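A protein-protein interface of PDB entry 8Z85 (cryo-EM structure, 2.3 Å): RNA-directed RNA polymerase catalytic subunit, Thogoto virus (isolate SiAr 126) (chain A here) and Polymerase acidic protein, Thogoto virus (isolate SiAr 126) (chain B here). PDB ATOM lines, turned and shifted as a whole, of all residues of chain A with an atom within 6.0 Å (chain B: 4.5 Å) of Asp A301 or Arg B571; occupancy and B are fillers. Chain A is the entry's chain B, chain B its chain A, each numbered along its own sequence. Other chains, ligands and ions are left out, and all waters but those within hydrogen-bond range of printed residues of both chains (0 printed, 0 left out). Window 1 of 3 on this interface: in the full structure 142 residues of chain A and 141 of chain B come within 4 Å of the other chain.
NE2 of Gln A16 lies within hydrogen-bond range of O of Arg B570, at 3.4 Å. The guanidinium group (NH2) of Arg B571 is in salt-bridge range of the side-chain carboxylate (OD1) of Asp A301 (3.9 Å).
Asp A301 touches just one residue of chain B: Arg B571 (3.9 Å). Printed residues of chain B within 4 Å of Ser A457: Arg B571. Of the printed residues of chain A, Met B574 touches Gln A16 and Ile A460. Of the printed residues of chain B, Lys A458 touches Asn B568 and Arg B571. Printed residues of chain B within 4 Å of Gln A16: Arg B570, His B573 and Met B574. Printed residues of chain A within 4 Å of Ser B575: Ile A460 (3.9 Å). The nearest printed residue of chain B that does not touch Asp A301 is Asn B568 (7.4 Å). The nearest residue of chain A that does not touch Arg B571 is Ile A460 (4.3 Å). The nearest printed residue of chain A that does not touch Asn B568 is Ser A457 (6.4 Å).
Printed residues of chain B that touch a printed residue of chain A: Asn B568, Arg B570, Arg B571, His B573, Met B574 and Ser B575. Hydrophobic or aromatic side chains of chain B within 4 Å of the printed part of chain A: His B573 and Met B574. Hydrophobic or aromatic side chains of chain A within 4 Å of the printed part of chain B: Ile A460. Among the printed residues, 9 pairs touch across the chains.
The side-chain amide oxygen (OD1) of Asn B568 sits at hydrogen-bond distance from the guanidinium group (NH1) of Arg B571. The backbone carbonyl oxygen of Arg B571 lies within hydrogen-bond range of the side-chain hydroxyl of Ser B575. The backbone carbonyl oxygen (O) of Ser A299 lies within hydrogen-bond range of the backbone NH (N) of Ile A460 (2.7 Å). The backbone carbonyl oxygen (O) of Asp A301 is in hydrogen-bond range of the backbone NH (N) of Ser A455. The side-chain sulfur (SG) of Cys A459 lies within hydrogen-bond range of the backbone carbonyl oxygen (O) of Asp A301 (3.5 Å).
Gln A16 touches His B573. Gln A16 touches Met B574. O of Ser A457 touches CD of Arg B571, at 3.6 Å. Asn B568 touches Lys A458 (OD1 to CE, 3.9 Å). Arg B571 touches Lys A458. CE of Met B574 touches CG2 of Ile A460, 3.7 Å away. Ile A460 touches Ser B575 (CG2 to OG, 3.9 Å).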
ATOM      1  N   GLN A  16      15.969 -15.659   6.566  1.00  0.00           N
ATOM      2  CA  GLN A  16      15.325 -15.255   5.320  1.00  0.00           C
ATOM      3  C   GLN A  16      13.882 -15.733   5.248  1.00  0.00           C
ATOM      4  O   GLN A  16      13.048 -15.079   4.611  1.00  0.00           O
ATOM      5  CB  GLN A  16      16.115 -15.773   4.118  1.00  0.00           C
ATOM      6  CG  GLN A  16      17.452 -15.088   3.915  1.00  0.00           C
ATOM      7  CD  GLN A  16      17.347 -13.867   3.026  1.00  0.00           C
ATOM      8  OE1 GLN A  16      16.251 -13.447   2.659  1.00  0.00           O
ATOM      9  NE2 GLN A  16      18.488 -13.290   2.675  1.00  0.00           N
ATOM     10  N   SER A 299      23.486 -13.487  -8.214  1.00  0.00           N
ATOM     11  CA  SER A 299      22.091 -13.873  -8.065  1.00  0.00           C
ATOM     12  C   SER A 299      21.216 -12.755  -8.608  1.00  0.00           C
ATOM     13  O   SER A 299      21.405 -11.589  -8.249  1.00  0.00           O
ATOM     14  CB  SER A 299      21.746 -14.154  -6.600  1.00  0.00           C
ATOM     15  OG  SER A 299      22.630 -15.110  -6.042  1.00  0.00           O
ATOM     16  N   GLY A 300      20.264 -13.106  -9.464  1.00  0.00           N
ATOM     17  CA  GLY A 300      19.416 -12.084 -10.045  1.00  0.00           C
ATOM     18  C   GLY A 300      18.267 -12.689 -10.818  1.00  0.00           C
ATOM     19  O   GLY A 300      18.147 -13.909 -10.953  1.00  0.00           O
ATOM     20  N   ASP A 301      17.415 -11.804 -11.320  1.00  0.00           N
ATOM     21  CA  ASP A 301      16.270 -12.153 -12.147  1.00  0.00           C
ATOM     22  C   ASP A 301      16.361 -11.401 -13.470  1.00  0.00           C
ATOM     23  O   ASP A 301      17.283 -10.616 -13.705  1.00  0.00           O
ATOM     24  CB  ASP A 301      14.957 -11.835 -11.426  1.00  0.00           C
ATOM     25  CG  ASP A 301      14.904 -12.416 -10.027  1.00  0.00           C
ATOM     26  OD1 ASP A 301      15.628 -11.911  -9.145  1.00  0.00           O
ATOM     27  OD2 ASP A 301      14.137 -13.377  -9.811  1.00  0.00           O
ATOM     28  N   GLN A 302      15.389 -11.646 -14.342  1.00  0.00           N
ATOM     29  CA  GLN A 302      15.313 -10.995 -15.642  1.00  0.00           C
ATOM     30  C   GLN A 302      14.096 -10.081 -15.680  1.00  0.00           C
ATOM     31  O   GLN A 302      12.976 -10.524 -15.409  1.00  0.00           O
ATOM     32  CB  GLN A 302      15.235 -12.026 -16.771  1.00  0.00           C
ATOM     33  CG  GLN A 302      16.061 -13.282 -16.540  1.00  0.00           C
ATOM     34  CD  GLN A 302      17.526 -13.103 -16.891  1.00  0.00           C
ATOM     35  OE1 GLN A 302      18.011 -11.982 -17.036  1.00  0.00           O
ATOM     36  NE2 GLN A 302      18.237 -14.214 -17.036  1.00  0.00           N
ATOM     37  N   GLU A 303      14.319  -8.812 -16.012  1.00  0.00           N
ATOM     38  CA  GLU A 303      13.224  -7.863 -16.141  1.00  0.00           C
ATOM     39  C   GLU A 303      12.563  -8.003 -17.504  1.00  0.00           C
ATOM     40  O   GLU A 303      13.238  -8.187 -18.521  1.00  0.00           O
ATOM     41  CB  GLU A 303      13.720  -6.430 -15.945  1.00  0.00           C
ATOM     42  CG  GLU A 303      14.783  -5.990 -16.937  1.00  0.00           C
ATOM     43  CD  GLU A 303      15.115  -4.516 -16.822  1.00  0.00           C
ATOM     44  OE1 GLU A 303      14.343  -3.780 -16.172  1.00  0.00           O
ATOM     45  OE2 GLU A 303      16.145  -4.093 -17.386  1.00  0.00           O
ATOM     46  N   ASP A 422      12.760 -16.682 -15.556  1.00  0.00           N
ATOM     47  CA  ASP A 422      13.334 -15.386 -15.190  1.00  0.00           C
ATOM     48  C   ASP A 422      13.993 -15.428 -13.815  1.00  0.00           C
ATOM     49  O   ASP A 422      13.746 -14.584 -12.955  1.00  0.00           O
ATOM     50  CB  ASP A 422      12.258 -14.308 -15.250  1.00  0.00           C
ATOM     51  CG  ASP A 422      11.040 -14.650 -14.413  1.00  0.00           C
ATOM     52  OD1 ASP A 422      10.991 -15.766 -13.851  1.00  0.00           O
ATOM     53  OD2 ASP A 422      10.132 -13.800 -14.314  1.00  0.00           O
ATOM     54  N   ASP A 423      14.858 -16.416 -13.608  1.00  0.00           N
ATOM     55  CA  ASP A 423      15.568 -16.567 -12.346  1.00  0.00           C
ATOM     56  C   ASP A 423      16.820 -17.386 -12.604  1.00  0.00           C
ATOM     57  O   ASP A 423      16.735 -18.488 -13.151  1.00  0.00           O
ATOM     58  CB  ASP A 423      14.694 -17.245 -11.288  1.00  0.00           C
ATOM     59  CG  ASP A 423      15.174 -16.970  -9.877  1.00  0.00           C
ATOM     60  OD1 ASP A 423      16.040 -16.089  -9.700  1.00  0.00           O
ATOM     61  OD2 ASP A 423      14.684 -17.638  -8.943  1.00  0.00           O
ATOM     62  N   PHE A 424      17.972 -16.850 -12.210  1.00  0.00           N
ATOM     63  CA  PHE A 424      19.238 -17.485 -12.530  1.00  0.00           C
ATOM     64  C   PHE A 424      20.234 -17.246 -11.407  1.00  0.00           C
ATOM     65  O   PHE A 424      20.096 -16.316 -10.609  1.00  0.00           O
ATOM     66  CB  PHE A 424      19.797 -16.965 -13.860  1.00  0.00           C
ATOM     67  CG  PHE A 424      20.371 -15.582 -13.777  1.00  0.00           C
ATOM     68  CD1 PHE A 424      19.557 -14.474 -13.934  1.00  0.00           C
ATOM     69  CD2 PHE A 424      21.724 -15.388 -13.560  1.00  0.00           C
ATOM     70  CE1 PHE A 424      20.077 -13.204 -13.858  1.00  0.00           C
ATOM     71  CE2 PHE A 424      22.249 -14.119 -13.483  1.00  0.00           C
ATOM     72  CZ  PHE A 424      21.424 -13.028 -13.633  1.00  0.00           C
ATOM     73  N   ASN A 453      16.908  -9.547 -20.747  1.00  0.00           N
ATOM     74  CA  ASN A 453      17.547  -8.438 -20.055  1.00  0.00           C
ATOM     75  C   ASN A 453      17.625  -8.750 -18.568  1.00  0.00           C
ATOM     76  O   ASN A 453      16.605  -9.049 -17.939  1.00  0.00           O
ATOM     77  CB  ASN A 453      16.779  -7.137 -20.285  1.00  0.00           C
ATOM     78  CG  ASN A 453      16.473  -6.894 -21.746  1.00  0.00           C
ATOM     79  OD1 ASN A 453      17.253  -6.267 -22.461  1.00  0.00           O
ATOM     80  ND2 ASN A 453      15.326  -7.382 -22.197  1.00  0.00           N
ATOM     81  N   MET A 454      18.832  -8.681 -18.013  1.00  0.00           N
ATOM     82  CA  MET A 454      18.992  -8.735 -16.568  1.00  0.00           C
ATOM     83  C   MET A 454      18.356  -7.511 -15.925  1.00  0.00           C
ATOM     84  O   MET A 454      18.488  -6.390 -16.423  1.00  0.00           O
ATOM     85  CB  MET A 454      20.473  -8.806 -16.198  1.00  0.00           C
ATOM     86  CG  MET A 454      21.177 -10.087 -16.606  1.00  0.00           C
ATOM     87  SD  MET A 454      22.940 -10.055 -16.219  1.00  0.00           S
ATOM     88  CE  MET A 454      22.937 -10.151 -14.437  1.00  0.00           C
ATOM     89  N   SER A 455      17.656  -7.729 -14.817  1.00  0.00           N
ATOM     90  CA  SER A 455      17.098  -6.612 -14.068  1.00  0.00           C
ATOM     91  C   SER A 455      18.213  -5.976 -13.249  1.00  0.00           C
ATOM     92  O   SER A 455      18.761  -6.620 -12.347  1.00  0.00           O
ATOM     93  CB  SER A 455      15.954  -7.076 -13.167  1.00  0.00           C
ATOM     94  OG  SER A 455      15.348  -5.981 -12.503  1.00  0.00           O
ATOM     95  N   SER A 457      18.310  -3.750 -10.861  1.00  0.00           N
ATOM     96  CA  SER A 457      18.052  -3.606  -9.435  1.00  0.00           C
ATOM     97  C   SER A 457      17.802  -4.935  -8.736  1.00  0.00           C
ATOM     98  O   SER A 457      17.686  -4.953  -7.506  1.00  0.00           O
ATOM     99  CB  SER A 457      16.858  -2.676  -9.215  1.00  0.00           C
ATOM    100  OG  SER A 457      17.053  -1.438  -9.874  1.00  0.00           O
ATOM    101  N   LYS A 458      17.721  -6.037  -9.477  1.00  0.00           N
ATOM    102  CA  LYS A 458      17.444  -7.343  -8.899  1.00  0.00           C
ATOM    103  C   LYS A 458      18.619  -8.304  -8.998  1.00  0.00           C
ATOM    104  O   LYS A 458      18.513  -9.438  -8.520  1.00  0.00           O
ATOM    105  CB  LYS A 458      16.214  -7.963  -9.570  1.00  0.00           C
ATOM    106  CG  LYS A 458      14.916  -7.240  -9.258  1.00  0.00           C
ATOM    107  CD  LYS A 458      13.723  -8.172  -9.350  1.00  0.00           C
ATOM    108  CE  LYS A 458      12.434  -7.388  -9.531  1.00  0.00           C
ATOM    109  NZ  LYS A 458      11.244  -8.281  -9.594  1.00  0.00           N
ATOM    110  N   CYS A 459      19.732  -7.888  -9.596  1.00  0.00           N
ATOM    111  CA  CYS A 459      20.910  -8.732  -9.751  1.00  0.00           C
ATOM    112  C   CYS A 459      21.996  -8.254  -8.796  1.00  0.00           C
ATOM    113  O   CYS A 459      22.401  -7.088  -8.844  1.00  0.00           O
ATOM    114  CB  CYS A 459      21.411  -8.717 -11.194  1.00  0.00           C
ATOM    115  SG  CYS A 459      20.215  -9.351 -12.390  1.00  0.00           S
ATOM    116  N   ILE A 460      22.464  -9.156  -7.938  1.00  0.00           N
ATOM    117  CA  ILE A 460      23.465  -8.851  -6.923  1.00  0.00           C
ATOM    118  C   ILE A 460      24.649  -9.780  -7.137  1.00  0.00           C
ATOM    119  O   ILE A 460      24.475 -10.999  -7.244  1.00  0.00           O
ATOM    120  CB  ILE A 460      22.898  -9.016  -5.500  1.00  0.00           C
ATOM    121  CG1 ILE A 460      21.657  -8.143  -5.303  1.00  0.00           C
ATOM    122  CG2 ILE A 460      23.949  -8.655  -4.469  1.00  0.00           C
ATOM    123  CD1 ILE A 460      21.913  -6.671  -5.437  1.00  0.00           C
ATOM    124  N   GLU A 469      21.050 -16.559  -3.785  1.00  0.00           N
ATOM    125  CA  GLU A 469      19.688 -17.069  -3.748  1.00  0.00           C
ATOM    126  C   GLU A 469      19.242 -17.430  -5.157  1.00  0.00           C
ATOM    127  O   GLU A 469      19.618 -16.775  -6.132  1.00  0.00           O
ATOM    128  CB  GLU A 469      18.720 -16.051  -3.124  1.00  0.00           C
ATOM    129  CG  GLU A 469      18.663 -14.710  -3.842  1.00  0.00           C
ATOM    130  CD  GLU A 469      17.574 -14.652  -4.896  1.00  0.00           C
ATOM    131  OE1 GLU A 469      16.632 -15.470  -4.826  1.00  0.00           O
ATOM    132  OE2 GLU A 469      17.660 -13.789  -5.794  1.00  0.00           O
ATOM    133  N   ALA B 567       9.376  -9.301  -0.697  1.00  0.00           N
ATOM    134  CA  ALA B 567      10.016 -10.021  -1.794  1.00  0.00           C
ATOM    135  C   ALA B 567      11.274  -9.306  -2.270  1.00  0.00           C
ATOM    136  O   ALA B 567      12.302  -9.944  -2.523  1.00  0.00           O
ATOM    137  CB  ALA B 567       9.033 -10.200  -2.948  1.00  0.00           C
ATOM    138  N   ASN B 568      11.212  -7.983  -2.399  1.00  0.00           N
ATOM    139  CA  ASN B 568      12.375  -7.212  -2.810  1.00  0.00           C
ATOM    140  C   ASN B 568      13.304  -6.883  -1.651  1.00  0.00           C
ATOM    141  O   ASN B 568      14.411  -6.388  -1.887  1.00  0.00           O
ATOM    142  CB  ASN B 568      11.927  -5.922  -3.498  1.00  0.00           C
ATOM    143  CG  ASN B 568      11.179  -6.184  -4.787  1.00  0.00           C
ATOM    144  OD1 ASN B 568      11.753  -6.656  -5.767  1.00  0.00           O
ATOM    145  ND2 ASN B 568       9.885  -5.888  -4.791  1.00  0.00           N
ATOM    146  N   MET B 569      12.883  -7.141  -0.414  1.00  0.00           N
ATOM    147  CA  MET B 569      13.726  -6.886   0.744  1.00  0.00           C
ATOM    148  C   MET B 569      14.728  -8.006   0.990  1.00  0.00           C
ATOM    149  O   MET B 569      15.723  -7.789   1.689  1.00  0.00           O
ATOM    150  CB  MET B 569      12.853  -6.695   1.986  1.00  0.00           C
ATOM    151  CG  MET B 569      13.539  -5.985   3.127  1.00  0.00           C
ATOM    152  SD  MET B 569      13.804  -4.257   2.703  1.00  0.00           S
ATOM    153  CE  MET B 569      15.228  -3.884   3.708  1.00  0.00           C
ATOM    154  N   ARG B 570      14.487  -9.190   0.424  1.00  0.00           N
ATOM    155  CA  ARG B 570      15.335 -10.343   0.711  1.00  0.00           C
ATOM    156  C   ARG B 570      16.739 -10.163   0.148  1.00  0.00           C
ATOM    157  O   ARG B 570      17.721 -10.570   0.781  1.00  0.00           O
ATOM    158  CB  ARG B 570      14.686 -11.612   0.164  1.00  0.00           C
ATOM    159  CG  ARG B 570      13.510 -12.085   0.997  1.00  0.00           C
ATOM    160  CD  ARG B 570      12.754 -13.214   0.329  1.00  0.00           C
ATOM    161  NE  ARG B 570      11.320 -13.105   0.566  1.00  0.00           N
ATOM    162  CZ  ARG B 570      10.392 -13.265  -0.367  1.00  0.00           C
ATOM    163  NH1 ARG B 570      10.710 -13.556  -1.616  1.00  0.00           N
ATOM    164  NH2 ARG B 570       9.112 -13.126  -0.036  1.00  0.00           N
ATOM    165  N   ARG B 571      16.862  -9.568  -1.040  1.00  0.00           N
ATOM    166  CA  ARG B 571      18.190  -9.355  -1.608  1.00  0.00           C
ATOM    167  C   ARG B 571      18.966  -8.291  -0.841  1.00  0.00           C
ATOM    168  O   ARG B 571      20.190  -8.400  -0.707  1.00  0.00           O
ATOM    169  CB  ARG B 571      18.085  -8.996  -3.091  1.00  0.00           C
ATOM    170  CG  ARG B 571      17.400  -7.677  -3.394  1.00  0.00           C
ATOM    171  CD  ARG B 571      17.314  -7.449  -4.893  1.00  0.00           C
ATOM    172  NE  ARG B 571      16.522  -8.483  -5.550  1.00  0.00           N
ATOM    173  CZ  ARG B 571      15.214  -8.408  -5.758  1.00  0.00           C
ATOM    174  NH1 ARG B 571      14.518  -7.344  -5.395  1.00  0.00           N
ATOM    175  NH2 ARG B 571      14.592  -9.426  -6.346  1.00  0.00           N
ATOM    176  N   LEU B 572      18.283  -7.259  -0.338  1.00  0.00           N
ATOM    177  CA  LEU B 572      18.948  -6.296   0.533  1.00  0.00           C
ATOM    178  C   LEU B 572      19.365  -6.943   1.846  1.00  0.00           C
ATOM    179  O   LEU B 572      20.455  -6.670   2.361  1.00  0.00           O
ATOM    180  CB  LEU B 572      18.036  -5.096   0.788  1.00  0.00           C
ATOM    181  CG  LEU B 572      17.725  -4.215  -0.421  1.00  0.00           C
ATOM    182  CD1 LEU B 572      16.948  -2.981   0.004  1.00  0.00           C
ATOM    183  CD2 LEU B 572      19.003  -3.824  -1.139  1.00  0.00           C
ATOM    184  N   HIS B 573      18.506  -7.797   2.405  1.00  0.00           N
ATOM    185  CA  HIS B 573      18.876  -8.554   3.595  1.00  0.00           C
ATOM    186  C   HIS B 573      20.052  -9.478   3.309  1.00  0.00           C
ATOM    187  O   HIS B 573      20.955  -9.625   4.139  1.00  0.00           O
ATOM    188  CB  HIS B 573      17.673  -9.352   4.098  1.00  0.00           C
ATOM    189  CG  HIS B 573      17.796  -9.802   5.519  1.00  0.00           C
ATOM    190  ND1 HIS B 573      17.688 -11.124   5.893  1.00  0.00           N
ATOM    191  CD2 HIS B 573      18.013  -9.105   6.660  1.00  0.00           C
ATOM    192  CE1 HIS B 573      17.833 -11.223   7.201  1.00  0.00           C
ATOM    193  NE2 HIS B 573      18.033 -10.013   7.691  1.00  0.00           N
ATOM    194  N   MET B 574      20.051 -10.115   2.135  1.00  0.00           N
ATOM    195  CA  MET B 574      21.189 -10.931   1.729  1.00  0.00           C
ATOM    196  C   MET B 574      22.433 -10.076   1.525  1.00  0.00           C
ATOM    197  O   MET B 574      23.548 -10.506   1.844  1.00  0.00           O
ATOM    198  CB  MET B 574      20.842 -11.705   0.457  1.00  0.00           C
ATOM    199  CG  MET B 574      21.998 -12.476  -0.149  1.00  0.00           C
ATOM    200  SD  MET B 574      21.704 -12.942  -1.863  1.00  0.00           S
ATOM    201  CE  MET B 574      22.281 -11.476  -2.712  1.00  0.00           C
ATOM    202  N   SER B 575      22.263  -8.863   0.994  1.00  0.00           N
ATOM    203  CA  SER B 575      23.401  -7.968   0.808  1.00  0.00           C
ATOM    204  C   SER B 575      24.018  -7.567   2.140  1.00  0.00           C
ATOM    205  O   SER B 575      25.245  -7.465   2.258  1.00  0.00           O
ATOM    206  CB  SER B 575      22.971  -6.728   0.023  1.00  0.00           C
ATOM    207  OG  SER B 575      22.449  -7.081  -1.245  1.00  0.00           O
